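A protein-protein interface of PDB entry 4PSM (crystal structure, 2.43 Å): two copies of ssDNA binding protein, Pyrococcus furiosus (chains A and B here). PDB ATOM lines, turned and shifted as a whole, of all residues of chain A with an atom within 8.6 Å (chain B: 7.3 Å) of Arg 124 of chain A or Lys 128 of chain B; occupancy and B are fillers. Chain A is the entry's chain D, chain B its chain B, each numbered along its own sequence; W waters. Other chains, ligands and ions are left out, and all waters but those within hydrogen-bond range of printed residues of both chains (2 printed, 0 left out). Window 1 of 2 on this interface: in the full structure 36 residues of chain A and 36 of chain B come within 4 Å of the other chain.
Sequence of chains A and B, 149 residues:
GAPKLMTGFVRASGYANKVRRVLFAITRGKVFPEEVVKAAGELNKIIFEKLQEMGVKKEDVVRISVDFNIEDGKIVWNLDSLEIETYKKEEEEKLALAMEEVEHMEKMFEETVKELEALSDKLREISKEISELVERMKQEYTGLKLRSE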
ATOM      1  N   GLU A 117       8.038   3.577  -3.238  1.00  0.00           N
ATOM      2  CA  GLU A 117       8.167   4.984  -2.897  1.00  0.00           C
ATOM      3  C   GLU A 117       7.537   5.288  -1.541  1.00  0.00           C
ATOM      4  O   GLU A 117       8.076   6.062  -0.754  1.00  0.00           O
ATOM      5  CB  GLU A 117       7.513   5.855  -3.965  1.00  0.00           C
ATOM      6  CG  GLU A 117       7.619   7.346  -3.703  1.00  0.00           C
ATOM      7  CD  GLU A 117       6.807   8.179  -4.683  1.00  0.00           C
ATOM      8  OE1 GLU A 117       5.664   7.786  -4.996  1.00  0.00           O
ATOM      9  OE2 GLU A 117       7.314   9.225  -5.145  1.00  0.00           O
ATOM     10  N   ALA A 118       6.386   4.686  -1.281  1.00  0.00           N
ATOM     11  CA  ALA A 118       5.681   4.907  -0.040  1.00  0.00           C
ATOM     12  C   ALA A 118       6.563   4.417   1.107  1.00  0.00           C
ATOM     13  O   ALA A 118       6.740   5.090   2.125  1.00  0.00           O
ATOM     14  CB  ALA A 118       4.356   4.162  -0.060  1.00  0.00           C
ATOM     15  N   LEU A 119       7.130   3.237   0.918  1.00  0.00           N
ATOM     16  CA  LEU A 119       8.021   2.652   1.900  1.00  0.00           C
ATOM     17  C   LEU A 119       9.223   3.551   2.170  1.00  0.00           C
ATOM     18  O   LEU A 119       9.599   3.769   3.325  1.00  0.00           O
ATOM     19  CB  LEU A 119       8.472   1.278   1.415  1.00  0.00           C
ATOM     20  CG  LEU A 119       7.754   0.048   1.975  1.00  0.00           C
ATOM     21  CD1 LEU A 119       6.491   0.323   2.780  1.00  0.00           C
ATOM     22  CD2 LEU A 119       7.633  -1.140   1.019  1.00  0.00           C
ATOM     23  N   SER A 120       9.821   4.077   1.108  1.00  0.00           N
ATOM     24  CA  SER A 120      11.021   4.894   1.251  1.00  0.00           C
ATOM     25  C   SER A 120      10.677   6.209   1.926  1.00  0.00           C
ATOM     26  O   SER A 120      11.498   6.772   2.645  1.00  0.00           O
ATOM     27  CB  SER A 120      11.681   5.158  -0.105  1.00  0.00           C
ATOM     28  OG  SER A 120      10.913   6.072  -0.871  1.00  0.00           O
ATOM     29  N   ASP A 121       9.461   6.694   1.681  1.00  0.00           N
ATOM     30  CA  ASP A 121       8.985   7.921   2.306  1.00  0.00           C
ATOM     31  C   ASP A 121       8.844   7.720   3.809  1.00  0.00           C
ATOM     32  O   ASP A 121       9.344   8.523   4.595  1.00  0.00           O
ATOM     33  CB  ASP A 121       7.651   8.373   1.703  1.00  0.00           C
ATOM     34  CG  ASP A 121       7.811   9.007   0.321  1.00  0.00           C
ATOM     35  OD1 ASP A 121       8.965   9.252  -0.096  1.00  0.00           O
ATOM     36  OD2 ASP A 121       6.781   9.269  -0.344  1.00  0.00           O
ATOM     37  N   LYS A 122       8.158   6.647   4.195  1.00  0.00           N
ATOM     38  CA  LYS A 122       8.026   6.272   5.591  1.00  0.00           C
ATOM     39  C   LYS A 122       9.419   6.170   6.196  1.00  0.00           C
ATOM     40  O   LYS A 122       9.693   6.726   7.257  1.00  0.00           O
ATOM     41  CB  LYS A 122       7.294   4.934   5.722  1.00  0.00           C
ATOM     42  CG  LYS A 122       5.782   5.002   5.535  1.00  0.00           C
ATOM     43  CD  LYS A 122       5.129   3.657   5.839  1.00  0.00           C
ATOM     44  CE  LYS A 122       3.612   3.726   5.705  1.00  0.00           C
ATOM     45  NZ  LYS A 122       2.963   2.413   5.976  1.00  0.00           N
ATOM     46  N   LEU A 123      10.302   5.474   5.491  1.00  0.00           N
ATOM     47  CA  LEU A 123      11.666   5.292   5.951  1.00  0.00           C
ATOM     48  C   LEU A 123      12.358   6.630   6.188  1.00  0.00           C
ATOM     49  O   LEU A 123      13.039   6.810   7.199  1.00  0.00           O
ATOM     50  CB  LEU A 123      12.466   4.454   4.948  1.00  0.00           C
ATOM     51  CG  LEU A 123      13.982   4.414   5.157  1.00  0.00           C
ATOM     52  CD1 LEU A 123      14.320   3.904   6.548  1.00  0.00           C
ATOM     53  CD2 LEU A 123      14.657   3.560   4.096  1.00  0.00           C
ATOM     54  N   ARG A 124      12.188   7.567   5.259  1.00  0.00           N
ATOM     55  CA  ARG A 124      12.881   8.842   5.372  1.00  0.00           C
ATOM     56  C   ARG A 124      12.379   9.547   6.622  1.00  0.00           C
ATOM     57  O   ARG A 124      13.156  10.127   7.383  1.00  0.00           O
ATOM     58  CB  ARG A 124      12.660   9.717   4.127  1.00  0.00           C
ATOM     59  CG  ARG A 124      13.535  10.968   4.096  1.00  0.00           C
ATOM     60  CD  ARG A 124      13.255  11.859   2.889  1.00  0.00           C
ATOM     61  NE  ARG A 124      13.991  13.122   2.970  1.00  0.00           N
ATOM     62  CZ  ARG A 124      15.143  13.365   2.351  1.00  0.00           C
ATOM     63  NH1 ARG A 124      15.701  12.437   1.586  1.00  0.00           N
ATOM     64  NH2 ARG A 124      15.738  14.544   2.495  1.00  0.00           N
ATOM     65  N   GLU A 125      11.070   9.468   6.836  1.00  0.00           N
ATOM     66  CA  GLU A 125      10.424  10.110   7.970  1.00  0.00           C
ATOM     67  C   GLU A 125      10.962   9.539   9.282  1.00  0.00           C
ATOM     68  O   GLU A 125      11.413  10.272  10.163  1.00  0.00           O
ATOM     69  CB  GLU A 125       8.912   9.902   7.883  1.00  0.00           C
ATOM     70  CG  GLU A 125       8.093  10.800   8.799  1.00  0.00           C
ATOM     71  CD  GLU A 125       6.598  10.635   8.587  1.00  0.00           C
ATOM     72  OE1 GLU A 125       6.137   9.478   8.478  1.00  0.00           O
ATOM     73  OE2 GLU A 125       5.889  11.661   8.516  1.00  0.00           O
ATOM     74  N   ILE A 126      10.916   8.219   9.395  1.00  0.00           N
ATOM     75  CA  ILE A 126      11.418   7.527  10.570  1.00  0.00           C
ATOM     76  C   ILE A 126      12.886   7.845  10.826  1.00  0.00           C
ATOM     77  O   ILE A 126      13.300   8.023  11.973  1.00  0.00           O
ATOM     78  CB  ILE A 126      11.245   6.010  10.421  1.00  0.00           C
ATOM     79  CG1 ILE A 126       9.855   5.596  10.888  1.00  0.00           C
ATOM     80  CG2 ILE A 126      12.304   5.257  11.205  1.00  0.00           C
ATOM     81  CD1 ILE A 126       9.595   4.126  10.718  1.00  0.00           C
ATOM     82  N   SER A 127      13.667   7.919   9.754  1.00  0.00           N
ATOM     83  CA  SER A 127      15.097   8.161   9.870  1.00  0.00           C
ATOM     84  C   SER A 127      15.334   9.551  10.439  1.00  0.00           C
ATOM     85  O   SER A 127      16.212   9.753  11.280  1.00  0.00           O
ATOM     86  CB  SER A 127      15.774   8.013   8.505  1.00  0.00           C
ATOM     87  OG  SER A 127      17.174   8.225   8.587  1.00  0.00           O
ATOM     88  N   LYS A 128      14.534  10.503   9.976  1.00  0.00           N
ATOM     89  CA  LYS A 128      14.630  11.872  10.444  1.00  0.00           C
ATOM     90  C   LYS A 128      14.251  11.953  11.921  1.00  0.00           C
ATOM     91  O   LYS A 128      14.922  12.620  12.709  1.00  0.00           O
ATOM     92  CB  LYS A 128      13.753  12.797   9.591  1.00  0.00           C
ATOM     93  CG  LYS A 128      14.392  13.179   8.255  1.00  0.00           C
ATOM     94  CD  LYS A 128      13.467  14.025   7.386  1.00  0.00           C
ATOM     95  CE  LYS A 128      14.148  14.421   6.079  1.00  0.00           C
ATOM     96  NZ  LYS A 128      13.258  15.206   5.168  1.00  0.00           N
ATOM     97  N   GLU A 129      13.179  11.262  12.291  1.00  0.00           N
ATOM     98  CA  GLU A 129      12.735  11.222  13.680  1.00  0.00           C
ATOM     99  C   GLU A 129      13.823  10.667  14.585  1.00  0.00           C
ATOM    100  O   GLU A 129      14.114  11.218  15.651  1.00  0.00           O
ATOM    101  CB  GLU A 129      11.471  10.377  13.820  1.00  0.00           C
ATOM    102  CG  GLU A 129      10.188  11.158  13.571  1.00  0.00           C
ATOM    103  CD  GLU A 129       8.957  10.274  13.593  1.00  0.00           C
ATOM    104  OE1 GLU A 129       8.822   9.414  12.694  1.00  0.00           O
ATOM    105  OE2 GLU A 129       8.125  10.436  14.512  1.00  0.00           O
ATOM    106  N   ILE A 130      14.424   9.570  14.151  1.00  0.00           N
ATOM    107  CA  ILE A 130      15.492   8.947  14.912  1.00  0.00           C
ATOM    108  C   ILE A 130      16.667   9.897  15.098  1.00  0.00           C
ATOM    109  O   ILE A 130      17.214   9.998  16.194  1.00  0.00           O
ATOM    110  CB  ILE A 130      15.944   7.630  14.265  1.00  0.00           C
ATOM    111  CG1 ILE A 130      14.898   6.550  14.532  1.00  0.00           C
ATOM    112  CG2 ILE A 130      17.288   7.188  14.816  1.00  0.00           C
ATOM    113  CD1 ILE A 130      15.078   5.296  13.690  1.00  0.00           C
ATOM    114  N   SER A 131      17.039  10.597  14.030  1.00  0.00           N
ATOM    115  CA  SER A 131      18.133  11.557  14.087  1.00  0.00           C
ATOM    116  C   SER A 131      17.820  12.685  15.052  1.00  0.00           C
ATOM    117  O   SER A 131      18.705  13.174  15.754  1.00  0.00           O
ATOM    118  CB  SER A 131      18.426  12.124  12.700  1.00  0.00           C
ATOM    119  OG  SER A 131      19.088  11.159  11.906  1.00  0.00           O
ATOM    120  N   GLU A 132      16.553  13.089  15.081  1.00  0.00           N
ATOM    121  CA  GLU A 132      16.097  14.170  15.946  1.00  0.00           C
ATOM    122  C   GLU A 132      16.176  13.740  17.400  1.00  0.00           C
ATOM    123  O   GLU A 132      16.730  14.441  18.241  1.00  0.00           O
ATOM    124  CB  GLU A 132      14.652  14.536  15.614  1.00  0.00           C
ATOM    125  CG  GLU A 132      14.356  16.026  15.661  1.00  0.00           C
ATOM    126  CD  GLU A 132      14.098  16.593  14.283  1.00  0.00           C
ATOM    127  OE1 GLU A 132      14.269  15.835  13.304  1.00  0.00           O
ATOM    128  OE2 GLU A 132      13.723  17.784  14.181  1.00  0.00           O
ATOM    129  N   LYS B 122      24.446   6.492   9.737  1.00  0.00           N
ATOM    130  CA  LYS B 122      24.444   5.484   8.693  1.00  0.00           C
ATOM    131  C   LYS B 122      23.038   5.356   8.136  1.00  0.00           C
ATOM    132  O   LYS B 122      22.829   5.388   6.920  1.00  0.00           O
ATOM    133  CB  LYS B 122      24.922   4.135   9.235  1.00  0.00           C
ATOM    134  CG  LYS B 122      26.428   4.013   9.416  1.00  0.00           C
ATOM    135  CD  LYS B 122      26.816   2.597   9.839  1.00  0.00           C
ATOM    136  CE  LYS B 122      28.325   2.454  10.018  1.00  0.00           C
ATOM    137  NZ  LYS B 122      28.714   1.073  10.427  1.00  0.00           N
ATOM    138  N   LEU B 123      22.075   5.236   9.039  1.00  0.00           N
ATOM    139  CA  LEU B 123      20.678   5.119   8.657  1.00  0.00           C
ATOM    140  C   LEU B 123      20.217   6.290   7.800  1.00  0.00           C
ATOM    141  O   LEU B 123      19.508   6.093   6.819  1.00  0.00           O
ATOM    142  CB  LEU B 123      19.785   5.006   9.891  1.00  0.00           C
ATOM    143  CG  LEU B 123      18.277   5.143   9.648  1.00  0.00           C
ATOM    144  CD1 LEU B 123      17.791   4.104   8.653  1.00  0.00           C
ATOM    145  CD2 LEU B 123      17.501   5.038  10.950  1.00  0.00           C
ATOM    146  N   ARG B 124      20.600   7.508   8.175  1.00  0.00           N
ATOM    147  CA  ARG B 124      20.148   8.675   7.436  1.00  0.00           C
ATOM    148  C   ARG B 124      20.724   8.612   6.028  1.00  0.00           C
ATOM    149  O   ARG B 124      20.037   8.890   5.051  1.00  0.00           O
ATOM    150  CB  ARG B 124      20.558   9.978   8.135  1.00  0.00           C
ATOM    151  CG  ARG B 124      19.925  11.223   7.516  1.00  0.00           C
ATOM    152  CD  ARG B 124      20.411  12.514   8.172  1.00  0.00           C
ATOM    153  NE  ARG B 124      19.917  13.699   7.469  1.00  0.00           N
ATOM    154  CZ  ARG B 124      18.859  14.413   7.847  1.00  0.00           C
ATOM    155  NH1 ARG B 124      18.178  14.079   8.933  1.00  0.00           N
ATOM    156  NH2 ARG B 124      18.486  15.468   7.137  1.00  0.00           N
ATOM    157  N   GLU B 125      21.991   8.214   5.947  1.00  0.00           N
ATOM    158  CA  GLU B 125      22.694   8.120   4.681  1.00  0.00           C
ATOM    159  C   GLU B 125      22.002   7.113   3.766  1.00  0.00           C
ATOM    160  O   GLU B 125      21.653   7.433   2.632  1.00  0.00           O
ATOM    161  CB  GLU B 125      24.147   7.715   4.930  1.00  0.00           C
ATOM    162  CG  GLU B 125      25.073   7.910   3.738  1.00  0.00           C
ATOM    163  CD  GLU B 125      26.523   7.601   4.072  1.00  0.00           C
ATOM    164  OE1 GLU B 125      26.774   6.569   4.730  1.00  0.00           O
ATOM    165  OE2 GLU B 125      27.408   8.395   3.684  1.00  0.00           O
ATOM    166  N   ILE B 126      21.801   5.903   4.280  1.00  0.00           N
ATOM    167  CA  ILE B 126      21.146   4.833   3.545  1.00  0.00           C
ATOM    168  C   ILE B 126      19.749   5.229   3.096  1.00  0.00           C
ATOM    169  O   ILE B 126      19.330   4.897   1.992  1.00  0.00           O
ATOM    170  CB  ILE B 126      21.057   3.558   4.402  1.00  0.00           C
ATOM    171  CG1 ILE B 126      22.327   2.732   4.240  1.00  0.00           C
ATOM    172  CG2 ILE B 126      19.837   2.714   4.025  1.00  0.00           C
ATOM    173  CD1 ILE B 126      22.330   1.489   5.093  1.00  0.00           C
ATOM    174  N   SER B 127      19.030   5.935   3.963  1.00  0.00           N
ATOM    175  CA  SER B 127      17.666   6.350   3.668  1.00  0.00           C
ATOM    176  C   SER B 127      17.662   7.328   2.499  1.00  0.00           C
ATOM    177  O   SER B 127      16.815   7.253   1.605  1.00  0.00           O
ATOM    178  CB  SER B 127      17.032   6.990   4.898  1.00  0.00           C
ATOM    179  OG  SER B 127      15.689   7.376   4.666  1.00  0.00           O
ATOM    180  N   LYS B 128      18.620   8.246   2.518  1.00  0.00           N
ATOM    181  CA  LYS B 128      18.777   9.215   1.448  1.00  0.00           C
ATOM    182  C   LYS B 128      19.106   8.526   0.122  1.00  0.00           C
ATOM    183  O   LYS B 128      18.538   8.859  -0.915  1.00  0.00           O
ATOM    184  CB  LYS B 128      19.848  10.244   1.825  1.00  0.00           C
ATOM    185  CG  LYS B 128      19.343  11.310   2.787  1.00  0.00           C
ATOM    186  CD  LYS B 128      20.436  12.283   3.203  1.00  0.00           C
ATOM    187  CE  LYS B 128      19.877  13.361   4.122  1.00  0.00           C
ATOM    188  NZ  LYS B 128      20.924  14.310   4.598  1.00  0.00           N
ATOM    189  N   GLU B 129      20.017   7.560   0.170  1.00  0.00           N
ATOM    190  CA  GLU B 129      20.400   6.806  -1.013  1.00  0.00           C
ATOM    191  C   GLU B 129      19.198   6.076  -1.591  1.00  0.00           C
ATOM    192  O   GLU B 129      18.976   6.075  -2.805  1.00  0.00           O
ATOM    193  CB  GLU B 129      21.492   5.798  -0.676  1.00  0.00           C
ATOM    194  CG  GLU B 129      22.904   6.355  -0.748  1.00  0.00           C
ATOM    195  CD  GLU B 129      23.950   5.349  -0.289  1.00  0.00           C
ATOM    196  OE1 GLU B 129      23.960   5.003   0.912  1.00  0.00           O
ATOM    197  OE2 GLU B 129      24.758   4.901  -1.132  1.00  0.00           O
ATOM    198  N   ILE B 130      18.418   5.458  -0.713  1.00  0.00           N
ATOM    199  CA  ILE B 130      17.229   4.745  -1.152  1.00  0.00           C
ATOM    200  C   ILE B 130      16.248   5.686  -1.853  1.00  0.00           C
ATOM    201  O   ILE B 130      15.733   5.374  -2.922  1.00  0.00           O
ATOM    202  CB  ILE B 130      16.566   3.992   0.007  1.00  0.00           C
ATOM    203  CG1 ILE B 130      17.394   2.745   0.342  1.00  0.00           C
ATOM    204  CG2 ILE B 130      15.137   3.603  -0.360  1.00  0.00           C
ATOM    205  CD1 ILE B 130      17.009   2.067   1.628  1.00  0.00           C
ATOM    206  N   SER B 131      16.025   6.847  -1.256  1.00  0.00           N
ATOM    207  CA  SER B 131      15.130   7.855  -1.808  1.00  0.00           C
ATOM    208  C   SER B 131      15.601   8.329  -3.176  1.00  0.00           C
ATOM    209  O   SER B 131      14.794   8.581  -4.063  1.00  0.00           O
ATOM    210  CB  SER B 131      15.024   9.052  -0.851  1.00  0.00           C
ATOM    211  OG  SER B 131      14.236   8.712   0.271  1.00  0.00           O
ATOM    212  N   GLU B 132      16.916   8.452  -3.324  1.00  0.00           N
ATOM    213  CA  GLU B 132      17.528   8.872  -4.577  1.00  0.00           C
ATOM    214  C   GLU B 132      17.311   7.806  -5.637  1.00  0.00           C
ATOM    215  O   GLU B 132      16.829   8.094  -6.728  1.00  0.00           O
ATOM    216  CB  GLU B 132      19.027   9.082  -4.384  1.00  0.00           C
ATOM    217  CG  GLU B 132      19.591  10.288  -5.104  1.00  0.00           C
ATOM    218  CD  GLU B 132      20.002  11.383  -4.140  1.00  0.00           C
ATOM    219  OE1 GLU B 132      19.742  11.231  -2.927  1.00  0.00           O
ATOM    220  OE2 GLU B 132      20.587  12.390  -4.595  1.00  0.00           O
ATOM    221  N   LEU B 133      17.670   6.572  -5.299  1.00  0.00           N
ATOM    222  CA  LEU B 133      17.540   5.446  -6.208  1.00  0.00           C
ATOM    223  C   LEU B 133      16.093   5.272  -6.669  1.00  0.00           C
ATOM    224  O   LEU B 133      15.819   5.125  -7.861  1.00  0.00           O
ATOM    225  CB  LEU B 133      18.047   4.176  -5.529  1.00  0.00           C
ATOM    226  CG  LEU B 133      18.042   2.900  -6.371  1.00  0.00           C
ATOM    227  CD1 LEU B 133      18.464   3.201  -7.809  1.00  0.00           C
ATOM    228  CD2 LEU B 133      18.948   1.840  -5.741  1.00  0.00           C
ATOM    229  N   VAL B 134      15.172   5.301  -5.714  1.00  0.00           N
ATOM    230  CA  VAL B 134      13.756   5.173  -6.011  1.00  0.00           C
ATOM    231  C   VAL B 134      13.303   6.230  -7.007  1.00  0.00           C
ATOM    232  O   VAL B 134      12.659   5.915  -8.006  1.00  0.00           O
ATOM    233  CB  VAL B 134      12.904   5.238  -4.733  1.00  0.00           C
ATOM    234  CG1 VAL B 134      11.427   5.394  -5.072  1.00  0.00           C
ATOM    235  CG2 VAL B 134      13.133   3.976  -3.902  1.00  0.00           C
ATOM    236  N   ARG B 136      15.098   7.844  -9.062  1.00  0.00           N
ATOM    237  CA  ARG B 136      15.793   7.560 -10.309  1.00  0.00           C
ATOM    238  C   ARG B 136      15.043   6.488 -11.116  1.00  0.00           C
ATOM    239  O   ARG B 136      14.909   6.599 -12.334  1.00  0.00           O
ATOM    240  CB  ARG B 136      17.225   7.121 -10.002  1.00  0.00           C
ATOM    241  CG  ARG B 136      18.245   7.512 -11.042  1.00  0.00           C
ATOM    242  CD  ARG B 136      19.524   8.009 -10.386  1.00  0.00           C
ATOM    243  NE  ARG B 136      20.083   7.053  -9.479  1.00  0.00           N
ATOM    244  CZ  ARG B 136      20.465   7.166  -8.211  1.00  0.00           C
ATOM    245  NH1 ARG B 136      20.406   8.272  -7.473  1.00  0.00           N
ATOM    246  NH2 ARG B 136      20.944   6.059  -7.685  1.00  0.00           N
ATOM    247  N   ARG B 147       9.121  14.120  -8.641  1.00  0.00           N
ATOM    248  CA  ARG B 147       9.315  15.210  -7.688  1.00  0.00           C
ATOM    249  C   ARG B 147       9.774  16.476  -8.403  1.00  0.00           C
ATOM    250  O   ARG B 147       9.458  17.588  -7.982  1.00  0.00           O
ATOM    251  CB  ARG B 147      10.344  14.823  -6.619  1.00  0.00           C
ATOM    252  CG  ARG B 147       9.967  13.602  -5.804  1.00  0.00           C
ATOM    253  CD  ARG B 147       8.739  13.869  -4.949  1.00  0.00           C
ATOM    254  NE  ARG B 147       8.156  12.639  -4.421  1.00  0.00           N
ATOM    255  CZ  ARG B 147       8.582  12.021  -3.324  1.00  0.00           C
ATOM    256  NH1 ARG B 147       9.604  12.513  -2.636  1.00  0.00           N
ATOM    257  NH2 ARG B 147       7.988  10.908  -2.919  1.00  0.00           N
HETATM  258  O   HOH W   1      11.431   8.791  -0.442  1.00  0.00           O
HETATM  259  O   HOH W   2      14.230   6.636   2.406  1.00  0.00           O
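The side-chain hydroxyl (OG) of Ser 120 of chain A is in hydrogen-bond range of the backbone carbonyl oxygen (O) of Glu 117 of chain A (2.8 Å). O of Ser 127 of chain A lies within hydrogen-bond range of OG of Ser 131 of chain A, 3.3 Å away. OG of Ser 131 of chain B lies within hydrogen-bond range of O of Ser 127 of chain B.
Of the printed residues of chain B, Asp 121 of chain A touches Arg 147. Of the printed residues of chain B, Arg 124 of chain A touches Ser 127 and Lys 128. Of the printed residues of chain B, Lys 128 of chain A touches Arg 124. Glu 129 of chain A touches none of the printed residues of chain B. Ser 127 of chain B touches just these residues of chain A: Leu 123 (3.5 Å), Arg 124 (3.2 Å) and Ser 127 (3.9 Å). Of the printed residues of chain A, Lys 128 of chain B touches Arg 124. Printed residues of chain A within 4 Å of Ile 130 of chain B: Ser 120 and Leu 123. Of the printed residues of chain A, Arg 147 of chain B touches Glu 117 and Asp 121. The nearest printed residue of chain B that does not touch Arg 124 of chain A is Ser 131 of chain B (4.2 Å). The nearest printed residue of chain A that does not touch Lys 128 of chain B is Lys 128 of chain A (6.1 Å).
Leu 123 of chain A touches Ser 127 of chain B, and with the chains exchanged Ser 127 of chain A touches Leu 123 of chain B. Leu 123 of chain A touches Ile 130 of chain B, and with the chains exchanged Ile 130 of chain A touches Leu 123 of chain B. Arg 124 of chain A touches Ser 127 of chain B, and with the chains exchanged Ser 127 of chain A touches Arg 124 of chain B. Arg 124 of chain A touches Lys 128 of chain B, and with the chains exchanged Lys 128 of chain A touches Arg 124 of chain B. Positions printed for both chains: 122, 123, 124, 125, 126, 127, 128, 129, 130, 131 and 132. Of the 13 pairs that touch across the chains among the printed residues, 9 have their exchanged pair printed and touching as well.
The guanidinium group (NH2) of Arg 147 of chain B is in salt-bridge range of the side-chain carboxylate (OD2) of Asp 121 of chain A (3.3 Å). The side-chain carboxylate (OE2) of Glu 117 of chain A is in salt-bridge range of the guanidinium group (NH2) of Arg 147 of chain B, at 2.9 Å.
Of the 16 printed residues of chain A, 8 touch a printed residue of chain B. Among the printed residues, 13 pairs touch across the chains. Among the printed residues, Asp or Glu carboxylates within 4 Å of a Lys or Arg side-chain nitrogen of the other chain: Glu 117 of chain A with Arg 147 of chain B (2.9 Å) and Asp 121 of chain A with Arg 147 of chain B (3.3 Å).
Water W1 lies within hydrogen-bond range of the side-chain carboxylate of Asp 121 of chain A (2.5 Å), the side-chain hydroxyl of Ser 120 of chain A (2.8 Å) and the side-chain hydroxyl of Ser 131 of chain B (2.9 Å). Water W2 lies within hydrogen-bond range of the backbone carbonyl oxygen of Ser 120 of chain A, the backbone carbonyl oxygen of Ser 127 of chain B and the side-chain hydroxyl of Ser 131 of chain B.
Among the printed residues, pairs that only touch across the chains: Glu 117 of chain A with Val 134 of chain B (3.9 Å), Ser 120 of chain A with Ile 130 of chain B (3.8 Å), Leu 123 of chain A with Ser 127 of chain B (3.5 Å), Leu 123 of chain A with Ile 130 of chain B (3.7 Å), Arg 124 of chain A with Ser 127 of chain B (3.2 Å), Arg 124 of chain A with Lys 128 of chain B (3.997 Å), Ser 127 of chain A with Leu 123 of chain B (3.4 Å), Ser 127 of chain A with Arg 124 of chain B (3.2 Å), Ser 127 of chain A with Ser 127 of chain B (3.9 Å), Lys 128 of chain A with Arg 124 of chain B (3.95 Å) and Ile 130 of chain A with Leu 123 of chain B (3.7 Å).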
